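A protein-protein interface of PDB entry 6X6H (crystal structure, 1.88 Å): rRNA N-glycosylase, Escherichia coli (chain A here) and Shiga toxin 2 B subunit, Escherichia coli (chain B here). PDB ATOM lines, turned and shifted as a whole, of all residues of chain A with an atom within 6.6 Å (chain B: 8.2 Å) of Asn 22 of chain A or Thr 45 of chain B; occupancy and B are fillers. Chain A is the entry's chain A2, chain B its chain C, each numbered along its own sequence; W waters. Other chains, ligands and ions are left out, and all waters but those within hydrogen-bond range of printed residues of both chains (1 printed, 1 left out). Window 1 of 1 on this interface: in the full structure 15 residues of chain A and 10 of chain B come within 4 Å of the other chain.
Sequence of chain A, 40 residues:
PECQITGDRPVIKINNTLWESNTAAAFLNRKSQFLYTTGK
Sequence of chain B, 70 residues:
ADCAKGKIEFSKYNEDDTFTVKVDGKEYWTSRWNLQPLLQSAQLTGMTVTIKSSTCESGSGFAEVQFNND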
ATOM      1  N   GLN A   4      30.971 -15.857 -11.636  1.00  0.00           N
ATOM      2  CA  GLN A   4      29.828 -15.480 -12.453  1.00  0.00           C
ATOM      3  C   GLN A   4      29.668 -16.448 -13.614  1.00  0.00           C
ATOM      4  O   GLN A   4      30.648 -16.780 -14.291  1.00  0.00           O
ATOM      5  CB  GLN A   4      29.989 -14.055 -12.978  1.00  0.00           C
ATOM      6  CG  GLN A   4      28.867 -13.585 -13.887  1.00  0.00           C
ATOM      7  CD  GLN A   4      29.212 -12.273 -14.566  1.00  0.00           C
ATOM      8  OE1 GLN A   4      30.225 -11.641 -14.245  1.00  0.00           O
ATOM      9  NE2 GLN A   4      28.379 -11.858 -15.513  1.00  0.00           N
ATOM     10  N   ILE A   5      28.433 -16.896 -13.837  1.00  0.00           N
ATOM     11  CA  ILE A   5      28.074 -17.633 -15.044  1.00  0.00           C
ATOM     12  C   ILE A   5      27.593 -16.625 -16.082  1.00  0.00           C
ATOM     13  O   ILE A   5      28.260 -16.399 -17.099  1.00  0.00           O
ATOM     14  CB  ILE A   5      26.997 -18.700 -14.770  1.00  0.00           C
ATOM     15  CG1 ILE A   5      27.529 -19.781 -13.830  1.00  0.00           C
ATOM     16  CG2 ILE A   5      26.527 -19.351 -16.071  1.00  0.00           C
ATOM     17  CD1 ILE A   5      26.569 -20.940 -13.659  1.00  0.00           C
ATOM     18  N   THR A   6      26.424 -16.030 -15.838  1.00  0.00           N
ATOM     19  CA  THR A   6      25.874 -14.977 -16.681  1.00  0.00           C
ATOM     20  C   THR A   6      25.197 -13.935 -15.799  1.00  0.00           C
ATOM     21  O   THR A   6      24.855 -14.195 -14.643  1.00  0.00           O
ATOM     22  CB  THR A   6      24.852 -15.504 -17.705  1.00  0.00           C
ATOM     23  OG1 THR A   6      23.612 -15.784 -17.044  1.00  0.00           O
ATOM     24  CG2 THR A   6      25.343 -16.768 -18.376  1.00  0.00           C
ATOM     25  N   GLY A   7      24.989 -12.749 -16.368  1.00  0.00           N
ATOM     26  CA  GLY A   7      24.280 -11.705 -15.663  1.00  0.00           C
ATOM     27  C   GLY A   7      25.125 -11.021 -14.606  1.00  0.00           C
ATOM     28  O   GLY A   7      26.339 -11.204 -14.512  1.00  0.00           O
ATOM     29  N   ASP A   8      24.451 -10.210 -13.790  1.00  0.00           N
ATOM     30  CA  ASP A   8      25.140  -9.393 -12.799  1.00  0.00           C
ATOM     31  C   ASP A   8      24.426  -9.363 -11.452  1.00  0.00           C
ATOM     32  O   ASP A   8      24.804  -8.563 -10.587  1.00  0.00           O
ATOM     33  CB  ASP A   8      25.328  -7.951 -13.318  1.00  0.00           C
ATOM     34  CG  ASP A   8      24.028  -7.145 -13.336  1.00  0.00           C
ATOM     35  OD1 ASP A   8      22.933  -7.744 -13.347  1.00  0.00           O
ATOM     36  OD2 ASP A   8      24.097  -5.900 -13.342  1.00  0.00           O
ATOM     37  N   ARG A   9      23.416 -10.195 -11.243  1.00  0.00           N
ATOM     38  CA  ARG A   9      22.651 -10.165 -10.003  1.00  0.00           C
ATOM     39  C   ARG A   9      22.915 -11.441  -9.223  1.00  0.00           C
ATOM     40  O   ARG A   9      22.395 -12.507  -9.594  1.00  0.00           O
ATOM     41  CB  ARG A   9      21.158 -10.014 -10.304  1.00  0.00           C
ATOM     42  CG  ARG A   9      20.259  -9.970  -9.078  1.00  0.00           C
ATOM     43  CD  ARG A   9      18.791  -9.950  -9.515  1.00  0.00           C
ATOM     44  NE  ARG A   9      17.871  -9.609  -8.431  1.00  0.00           N
ATOM     45  CZ  ARG A   9      16.563  -9.410  -8.594  1.00  0.00           C
ATOM     46  NH1 ARG A   9      16.009  -9.520  -9.803  1.00  0.00           N
ATOM     47  NH2 ARG A   9      15.804  -9.102  -7.548  1.00  0.00           N
ATOM     48  N   PRO A  10      23.712 -11.398  -8.152  1.00  0.00           N
ATOM     49  CA  PRO A  10      24.079 -12.657  -7.477  1.00  0.00           C
ATOM     50  C   PRO A  10      22.887 -13.452  -6.959  1.00  0.00           C
ATOM     51  O   PRO A  10      22.818 -14.673  -7.172  1.00  0.00           O
ATOM     52  CB  PRO A  10      24.996 -12.180  -6.340  1.00  0.00           C
ATOM     53  CG  PRO A  10      25.569 -10.887  -6.842  1.00  0.00           C
ATOM     54  CD  PRO A  10      24.471 -10.243  -7.635  1.00  0.00           C
ATOM     55  N   ILE A  12      18.485 -13.577  -5.522  1.00  0.00           N
ATOM     56  CA  ILE A  12      17.124 -13.067  -5.400  1.00  0.00           C
ATOM     57  C   ILE A  12      16.547 -13.670  -4.128  1.00  0.00           C
ATOM     58  O   ILE A  12      16.588 -14.892  -3.945  1.00  0.00           O
ATOM     59  CB  ILE A  12      16.247 -13.432  -6.613  1.00  0.00           C
ATOM     60  CG1 ILE A  12      16.848 -12.873  -7.904  1.00  0.00           C
ATOM     61  CG2 ILE A  12      14.833 -12.903  -6.429  1.00  0.00           C
ATOM     62  CD1 ILE A  12      16.068 -13.252  -9.157  1.00  0.00           C
ATOM     63  N   TRP A  19      17.964 -17.335  -3.302  1.00  0.00           N
ATOM     64  CA  TRP A  19      18.189 -18.081  -4.534  1.00  0.00           C
ATOM     65  C   TRP A  19      19.318 -17.463  -5.351  1.00  0.00           C
ATOM     66  O   TRP A  19      19.367 -16.243  -5.524  1.00  0.00           O
ATOM     67  CB  TRP A  19      16.938 -18.092  -5.415  1.00  0.00           C
ATOM     68  CG  TRP A  19      15.830 -18.945  -4.909  1.00  0.00           C
ATOM     69  CD1 TRP A  19      14.899 -18.619  -3.958  1.00  0.00           C
ATOM     70  CD2 TRP A  19      15.513 -20.265  -5.351  1.00  0.00           C
ATOM     71  NE1 TRP A  19      14.026 -19.672  -3.776  1.00  0.00           N
ATOM     72  CE2 TRP A  19      14.388 -20.694  -4.614  1.00  0.00           C
ATOM     73  CE3 TRP A  19      16.076 -21.133  -6.292  1.00  0.00           C
ATOM     74  CZ2 TRP A  19      13.820 -21.951  -4.792  1.00  0.00           C
ATOM     75  CZ3 TRP A  19      15.511 -22.387  -6.461  1.00  0.00           C
ATOM     76  CH2 TRP A  19      14.392 -22.780  -5.720  1.00  0.00           C
ATOM     77  N   GLU A  20      20.193 -18.307  -5.895  1.00  0.00           N
ATOM     78  CA  GLU A  20      21.006 -17.857  -7.022  1.00  0.00           C
ATOM     79  C   GLU A  20      20.075 -17.383  -8.135  1.00  0.00           C
ATOM     80  O   GLU A  20      19.171 -18.115  -8.544  1.00  0.00           O
ATOM     81  CB  GLU A  20      21.904 -18.986  -7.526  1.00  0.00           C
ATOM     82  CG  GLU A  20      22.773 -18.565  -8.700  1.00  0.00           C
ATOM     83  CD  GLU A  20      23.309 -19.744  -9.488  1.00  0.00           C
ATOM     84  OE1 GLU A  20      22.490 -20.546  -9.985  1.00  0.00           O
ATOM     85  OE2 GLU A  20      24.548 -19.868  -9.611  1.00  0.00           O
ATOM     86  N   SER A  21      20.294 -16.152  -8.615  1.00  0.00           N
ATOM     87  CA  SER A  21      19.349 -15.562  -9.560  1.00  0.00           C
ATOM     88  C   SER A  21      19.221 -16.416 -10.812  1.00  0.00           C
ATOM     89  O   SER A  21      18.112 -16.618 -11.325  1.00  0.00           O
ATOM     90  CB  SER A  21      19.773 -14.138  -9.929  1.00  0.00           C
ATOM     91  OG  SER A  21      19.890 -13.318  -8.779  1.00  0.00           O
ATOM     92  N   ASN A  22      20.346 -16.945 -11.305  1.00  0.00           N
ATOM     93  CA  ASN A  22      20.322 -17.750 -12.521  1.00  0.00           C
ATOM     94  C   ASN A  22      19.493 -19.022 -12.357  1.00  0.00           C
ATOM     95  O   ASN A  22      18.870 -19.472 -13.324  1.00  0.00           O
ATOM     96  CB  ASN A  22      21.749 -18.099 -12.954  1.00  0.00           C
ATOM     97  CG  ASN A  22      22.438 -16.949 -13.683  1.00  0.00           C
ATOM     98  OD1 ASN A  22      21.784 -16.082 -14.261  1.00  0.00           O
ATOM     99  ND2 ASN A  22      23.762 -16.953 -13.677  1.00  0.00           N
ATOM    100  N   THR A  23      19.466 -19.611 -11.155  1.00  0.00           N
ATOM    101  CA  THR A  23      18.640 -20.795 -10.940  1.00  0.00           C
ATOM    102  C   THR A  23      17.158 -20.441 -11.045  1.00  0.00           C
ATOM    103  O   THR A  23      16.402 -21.110 -11.756  1.00  0.00           O
ATOM    104  CB  THR A  23      18.952 -21.434  -9.578  1.00  0.00           C
ATOM    105  OG1 THR A  23      20.316 -21.862  -9.536  1.00  0.00           O
ATOM    106  CG2 THR A  23      18.057 -22.661  -9.339  1.00  0.00           C
ATOM    107  N   ALA A  24      16.740 -19.368 -10.370  1.00  0.00           N
ATOM    108  CA  ALA A  24      15.347 -18.931 -10.456  1.00  0.00           C
ATOM    109  C   ALA A  24      14.958 -18.584 -11.886  1.00  0.00           C
ATOM    110  O   ALA A  24      13.874 -18.965 -12.351  1.00  0.00           O
ATOM    111  CB  ALA A  24      15.108 -17.729  -9.541  1.00  0.00           C
ATOM    112  N   ALA A  25      15.834 -17.869 -12.606  1.00  0.00           N
ATOM    113  CA  ALA A  25      15.521 -17.486 -13.979  1.00  0.00           C
ATOM    114  C   ALA A  25      15.300 -18.697 -14.867  1.00  0.00           C
ATOM    115  O   ALA A  25      14.498 -18.639 -15.806  1.00  0.00           O
ATOM    116  CB  ALA A  25      16.647 -16.632 -14.565  1.00  0.00           C
ATOM    117  N   ALA A  26      15.996 -19.802 -14.581  1.00  0.00           N
ATOM    118  CA  ALA A  26      15.961 -20.995 -15.414  1.00  0.00           C
ATOM    119  C   ALA A  26      14.687 -21.821 -15.255  1.00  0.00           C
ATOM    120  O   ALA A  26      14.467 -22.737 -16.056  1.00  0.00           O
ATOM    121  CB  ALA A  26      17.178 -21.875 -15.109  1.00  0.00           C
ATOM    122  N   PHE A  27      13.853 -21.559 -14.246  1.00  0.00           N
ATOM    123  CA  PHE A  27      12.528 -22.172 -14.213  1.00  0.00           C
ATOM    124  C   PHE A  27      11.407 -21.154 -14.314  1.00  0.00           C
ATOM    125  O   PHE A  27      10.237 -21.551 -14.386  1.00  0.00           O
ATOM    126  CB  PHE A  27      12.321 -23.072 -12.971  1.00  0.00           C
ATOM    127  CG  PHE A  27      12.296 -22.355 -11.618  1.00  0.00           C
ATOM    128  CD1 PHE A  27      11.138 -21.744 -11.141  1.00  0.00           C
ATOM    129  CD2 PHE A  27      13.407 -22.405 -10.774  1.00  0.00           C
ATOM    130  CE1 PHE A  27      11.108 -21.129  -9.877  1.00  0.00           C
ATOM    131  CE2 PHE A  27      13.382 -21.796  -9.510  1.00  0.00           C
ATOM    132  CZ  PHE A  27      12.231 -21.161  -9.064  1.00  0.00           C
ATOM    133  N   LYS B   7      21.935  -4.609 -20.850  1.00  0.00           N
ATOM    134  CA  LYS B   7      20.900  -5.215 -20.025  1.00  0.00           C
ATOM    135  C   LYS B   7      19.546  -4.600 -20.342  1.00  0.00           C
ATOM    136  O   LYS B   7      19.452  -3.471 -20.823  1.00  0.00           O
ATOM    137  CB  LYS B   7      21.235  -5.038 -18.543  1.00  0.00           C
ATOM    138  CG  LYS B   7      22.560  -5.677 -18.157  1.00  0.00           C
ATOM    139  CD  LYS B   7      22.969  -5.323 -16.737  1.00  0.00           C
ATOM    140  CE  LYS B   7      24.399  -5.772 -16.458  1.00  0.00           C
ATOM    141  NZ  LYS B   7      25.414  -5.137 -17.356  1.00  0.00           N
ATOM    142  N   ILE B   8      18.487  -5.368 -20.088  1.00  0.00           N
ATOM    143  CA  ILE B   8      17.120  -4.909 -20.322  1.00  0.00           C
ATOM    144  C   ILE B   8      16.742  -3.942 -19.198  1.00  0.00           C
ATOM    145  O   ILE B   8      16.657  -4.334 -18.034  1.00  0.00           O
ATOM    146  CB  ILE B   8      16.147  -6.092 -20.401  1.00  0.00           C
ATOM    147  CG1 ILE B   8      16.485  -6.965 -21.619  1.00  0.00           C
ATOM    148  CG2 ILE B   8      14.700  -5.612 -20.469  1.00  0.00           C
ATOM    149  CD1 ILE B   8      15.943  -8.389 -21.550  1.00  0.00           C
ATOM    150  N   LEU B  38      11.677 -15.747 -22.255  1.00  0.00           N
ATOM    151  CA  LEU B  38      13.133 -15.781 -22.377  1.00  0.00           C
ATOM    152  C   LEU B  38      13.731 -14.410 -22.090  1.00  0.00           C
ATOM    153  O   LEU B  38      14.759 -14.302 -21.410  1.00  0.00           O
ATOM    154  CB  LEU B  38      13.545 -16.265 -23.774  1.00  0.00           C
ATOM    155  CG  LEU B  38      12.967 -17.589 -24.289  1.00  0.00           C
ATOM    156  CD1 LEU B  38      13.630 -18.015 -25.613  1.00  0.00           C
ATOM    157  CD2 LEU B  38      13.086 -18.695 -23.232  1.00  0.00           C
ATOM    158  N   LEU B  39      13.091 -13.347 -22.599  1.00  0.00           N
ATOM    159  CA  LEU B  39      13.548 -11.991 -22.327  1.00  0.00           C
ATOM    160  C   LEU B  39      13.338 -11.610 -20.865  1.00  0.00           C
ATOM    161  O   LEU B  39      14.179 -10.923 -20.272  1.00  0.00           O
ATOM    162  CB  LEU B  39      12.827 -10.996 -23.245  1.00  0.00           C
ATOM    163  CG  LEU B  39      13.158 -11.123 -24.734  1.00  0.00           C
ATOM    164  CD1 LEU B  39      12.179 -10.304 -25.584  1.00  0.00           C
ATOM    165  CD2 LEU B  39      14.606 -10.697 -25.002  1.00  0.00           C
ATOM    166  N   GLN B  40      12.217 -12.027 -20.267  1.00  0.00           N
ATOM    167  CA  GLN B  40      11.978 -11.625 -18.885  1.00  0.00           C
ATOM    168  C   GLN B  40      12.993 -12.267 -17.946  1.00  0.00           C
ATOM    169  O   GLN B  40      13.424 -11.643 -16.966  1.00  0.00           O
ATOM    170  CB  GLN B  40      10.546 -11.958 -18.449  1.00  0.00           C
ATOM    171  CG  GLN B  40      10.219 -11.362 -17.077  1.00  0.00           C
ATOM    172  CD  GLN B  40       8.927 -11.871 -16.480  1.00  0.00           C
ATOM    173  OE1 GLN B  40       8.606 -13.056 -16.574  1.00  0.00           O
ATOM    174  NE2 GLN B  40       8.176 -10.969 -15.844  1.00  0.00           N
ATOM    175  N   SER B  41      13.407 -13.507 -18.232  1.00  0.00           N
ATOM    176  CA  SER B  41      14.414 -14.135 -17.380  1.00  0.00           C
ATOM    177  C   SER B  41      15.788 -13.505 -17.590  1.00  0.00           C
ATOM    178  O   SER B  41      16.568 -13.381 -16.637  1.00  0.00           O
ATOM    179  CB  SER B  41      14.469 -15.648 -17.624  1.00  0.00           C
ATOM    180  OG  SER B  41      13.434 -16.299 -16.888  1.00  0.00           O
ATOM    181  N   ALA B  42      16.113 -13.107 -18.826  1.00  0.00           N
ATOM    182  CA  ALA B  42      17.333 -12.328 -19.036  1.00  0.00           C
ATOM    183  C   ALA B  42      17.286 -11.032 -18.239  1.00  0.00           C
ATOM    184  O   ALA B  42      18.279 -10.634 -17.626  1.00  0.00           O
ATOM    185  CB  ALA B  42      17.517 -12.024 -20.523  1.00  0.00           C
ATOM    186  N   GLN B  43      16.123 -10.380 -18.212  1.00  0.00           N
ATOM    187  CA  GLN B  43      15.985  -9.129 -17.476  1.00  0.00           C
ATOM    188  C   GLN B  43      16.217  -9.330 -15.983  1.00  0.00           C
ATOM    189  O   GLN B  43      16.958  -8.569 -15.346  1.00  0.00           O
ATOM    190  CB  GLN B  43      14.597  -8.530 -17.724  1.00  0.00           C
ATOM    191  CG  GLN B  43      14.336  -7.272 -16.906  1.00  0.00           C
ATOM    192  CD  GLN B  43      12.961  -6.684 -17.155  1.00  0.00           C
ATOM    193  OE1 GLN B  43      12.137  -7.280 -17.838  1.00  0.00           O
ATOM    194  NE2 GLN B  43      12.712  -5.494 -16.599  1.00  0.00           N
ATOM    195  N   LEU B  44      15.589 -10.349 -15.396  1.00  0.00           N
ATOM    196  CA  LEU B  44      15.646 -10.446 -13.942  1.00  0.00           C
ATOM    197  C   LEU B  44      17.031 -10.837 -13.437  1.00  0.00           C
ATOM    198  O   LEU B  44      17.349 -10.563 -12.274  1.00  0.00           O
ATOM    199  CB  LEU B  44      14.569 -11.410 -13.422  1.00  0.00           C
ATOM    200  CG  LEU B  44      14.595 -12.899 -13.742  1.00  0.00           C
ATOM    201  CD1 LEU B  44      15.409 -13.656 -12.686  1.00  0.00           C
ATOM    202  CD2 LEU B  44      13.160 -13.470 -13.829  1.00  0.00           C
ATOM    203  N   THR B  45      17.875 -11.429 -14.278  1.00  0.00           N
ATOM    204  CA  THR B  45      19.214 -11.816 -13.853  1.00  0.00           C
ATOM    205  C   THR B  45      20.296 -10.847 -14.316  1.00  0.00           C
ATOM    206  O   THR B  45      21.457 -11.015 -13.923  1.00  0.00           O
ATOM    207  CB  THR B  45      19.564 -13.230 -14.351  1.00  0.00           C
ATOM    208  OG1 THR B  45      20.619 -13.774 -13.550  1.00  0.00           O
ATOM    209  CG2 THR B  45      19.964 -13.215 -15.835  1.00  0.00           C
ATOM    210  N   GLY B  46      19.951  -9.847 -15.126  1.00  0.00           N
ATOM    211  CA  GLY B  46      20.932  -8.896 -15.616  1.00  0.00           C
ATOM    212  C   GLY B  46      21.703  -9.358 -16.830  1.00  0.00           C
ATOM    213  O   GLY B  46      22.820  -8.888 -17.060  1.00  0.00           O
ATOM    214  N   MET B  47      21.133 -10.262 -17.616  1.00  0.00           N
ATOM    215  CA  MET B  47      21.822 -10.818 -18.771  1.00  0.00           C
ATOM    216  C   MET B  47      22.002  -9.755 -19.852  1.00  0.00           C
ATOM    217  O   MET B  47      21.098  -8.965 -20.120  1.00  0.00           O
ATOM    218  CB  MET B  47      21.012 -11.999 -19.311  1.00  0.00           C
ATOM    219  CG  MET B  47      21.784 -13.036 -20.086  1.00  0.00           C
ATOM    220  SD  MET B  47      20.692 -14.388 -20.607  1.00  0.00           S
ATOM    221  CE  MET B  47      21.911 -15.681 -20.870  1.00  0.00           C
ATOM    222  N   THR B  48      23.184  -9.717 -20.457  1.00  0.00           N
ATOM    223  CA  THR B  48      23.416  -8.819 -21.580  1.00  0.00           C
ATOM    224  C   THR B  48      22.813  -9.422 -22.846  1.00  0.00           C
ATOM    225  O   THR B  48      23.135 -10.557 -23.207  1.00  0.00           O
ATOM    226  CB  THR B  48      24.910  -8.568 -21.769  1.00  0.00           C
ATOM    227  OG1 THR B  48      25.412  -7.803 -20.668  1.00  0.00           O
ATOM    228  CG2 THR B  48      25.153  -7.808 -23.065  1.00  0.00           C
ATOM    229  N   ASN B  68      23.829 -13.241 -24.150  1.00  0.00           N
ATOM    230  CA  ASN B  68      25.264 -13.359 -23.930  1.00  0.00           C
ATOM    231  C   ASN B  68      25.575 -13.710 -22.477  1.00  0.00           C
ATOM    232  O   ASN B  68      24.758 -13.517 -21.573  1.00  0.00           O
ATOM    233  CB  ASN B  68      25.978 -12.059 -24.313  1.00  0.00           C
ATOM    234  CG  ASN B  68      25.672 -11.619 -25.728  1.00  0.00           C
ATOM    235  OD1 ASN B  68      26.244 -12.138 -26.686  1.00  0.00           O
ATOM    236  ND2 ASN B  68      24.764 -10.650 -25.870  1.00  0.00           N
ATOM    237  N   ASN B  69      26.787 -14.217 -22.259  1.00  0.00           N
ATOM    238  CA  ASN B  69      27.230 -14.609 -20.929  1.00  0.00           C
ATOM    239  C   ASN B  69      27.965 -13.493 -20.196  1.00  0.00           C
ATOM    240  O   ASN B  69      28.534 -13.743 -19.131  1.00  0.00           O
ATOM    241  CB  ASN B  69      28.111 -15.855 -21.012  1.00  0.00           C
ATOM    242  CG  ASN B  69      27.306 -17.119 -21.271  1.00  0.00           C
ATOM    243  OD1 ASN B  69      26.082 -17.076 -21.423  1.00  0.00           O
ATOM    244  ND2 ASN B  69      27.992 -18.252 -21.322  1.00  0.00           N
ATOM    245  N   ASP B  70      27.968 -12.280 -20.743  1.00  0.00           N
ATOM    246  CA  ASP B  70      28.518 -11.109 -20.067  1.00  0.00           C
ATOM    247  C   ASP B  70      27.719 -10.748 -18.815  1.00  0.00           C
ATOM    248  O   ASP B  70      27.893 -11.347 -17.753  1.00  0.00           O
ATOM    249  CB  ASP B  70      28.537  -9.915 -21.020  1.00  0.00           C
ATOM    250  CG  ASP B  70      29.395 -10.161 -22.241  1.00  0.00           C
ATOM    251  OD1 ASP B  70      30.637 -10.140 -22.108  1.00  0.00           O
ATOM    252  OD2 ASP B  70      28.828 -10.394 -23.330  1.00  0.00           O
HETATM  253  O   HOH W   1      23.177 -13.254 -12.419  1.00  0.00           O
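N of Asp 8 of chain A sits at hydrogen-bond distance from O of Thr 45 of chain B, 3.1 Å away.
The guanidinium group (NH1) of Arg 9 of chain A sits at hydrogen-bond distance from the backbone carbonyl oxygen (O) of Leu 44 of chain B (3.0 Å).
O of Thr 45 of chain B is in hydrogen-bond range of N of Arg 9 of chain A (3.4 Å).
OD1 of Asn 22 of chain A sits at hydrogen-bond distance from OG1 of Thr 45 of chain B (2.7 Å).
OG of Ser 41 of chain B lies within hydrogen-bond range of O of Ala 25 of chain A, at 2.8 Å.
NE2 of Gln 4 of chain A lies close to O of Asp 70 of chain B.
The backbone carbonyl oxygen of Ile 5 of chain A sits close to the backbone carbonyl oxygen of Asn 69 of chain B (3.4 Å).
ND2 of Asn 22 of chain A sits at hydrogen-bond distance from O of Thr 6 of chain A.
The backbone carbonyl oxygen (O) of Arg 9 of chain A is in hydrogen-bond range of the side-chain hydroxyl (OG) of Ser 21 of chain A.
O of Pro 10 of chain A lies within hydrogen-bond range of N of Ser 21 of chain A (3.3 Å).
The backbone NH (N) of Ile 12 of chain A lies within hydrogen-bond range of the backbone carbonyl oxygen (O) of Trp 19 of chain A (2.8 Å).
The backbone carbonyl oxygen (O) of Ala 42 of chain B sits at hydrogen-bond distance from the backbone NH (N) of Met 47 of chain B, at 2.9 Å.
Among the printed residues, pairs that only touch across the chains: Asp 8 of chain A with Lys 7 of chain B (3.1 Å), Thr 6 of chain A with Asn 69 of chain B (3.2 Å), Asp 8 of chain A with Gly 46 of chain B (3.2 Å), Gly 7 of chain A with Thr 45 of chain B (3.4 Å), Gly 7 of chain A with Gly 46 of chain B (3.5 Å), Gly 7 of chain A with Asp 70 of chain B (3.5 Å), Ile 12 of chain A with Leu 44 of chain B (3.6 Å), Ala 25 of chain A with Leu 44 of chain B (3.7 Å), Ser 21 of chain A with Thr 45 of chain B (3.7 Å) and Gly 7 of chain A with Met 47 of chain B (3.97 Å).
Printed residues of chain B within 4 Å of Ser 21 of chain A: Thr 45 (3.7 Å).
Of the printed residues of chain B, Asn 22 of chain A touches Thr 45 (2.7 Å).
Ala 24 of chain A touches none of the printed residues of chain B.
Of the printed residues of chain A, Lys 7 of chain B touches Asp 8.
Printed residues of chain A within 4 Å of Thr 45 of chain B: Gly 7, Asp 8, Arg 9, Ser 21 and Asn 22.
Asn 68 of chain B touches none of the printed residues of chain A.
Of the printed residues of chain A, Asp 70 of chain B touches Gln 4 (2.3 Å) and Gly 7 (3.5 Å).
The nearest printed residue of chain B that does not touch Asn 22 of chain A is Leu 44 of chain B (6.1 Å).
The nearest printed residue of chain A that does not touch Thr 45 of chain B is Thr 6 of chain A (4.4 Å).
Of the 16 printed residues of chain B, 8 touch a printed residue of chain A.
Of the 17 printed residues of chain A, 10 touch a printed residue of chain B.
Hydrophobic or aromatic side chains of chain A within 4 Å of the printed part of chain B: Ile 12 and Ala 25.
Along chain A the printed residues that touch a printed residue of chain B span positions 4 to 25.
Water W1 lies within hydrogen-bond range of OG1 of Thr 45 of chain B, O of Thr 6 of chain A and O of Arg 9 of chain A.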
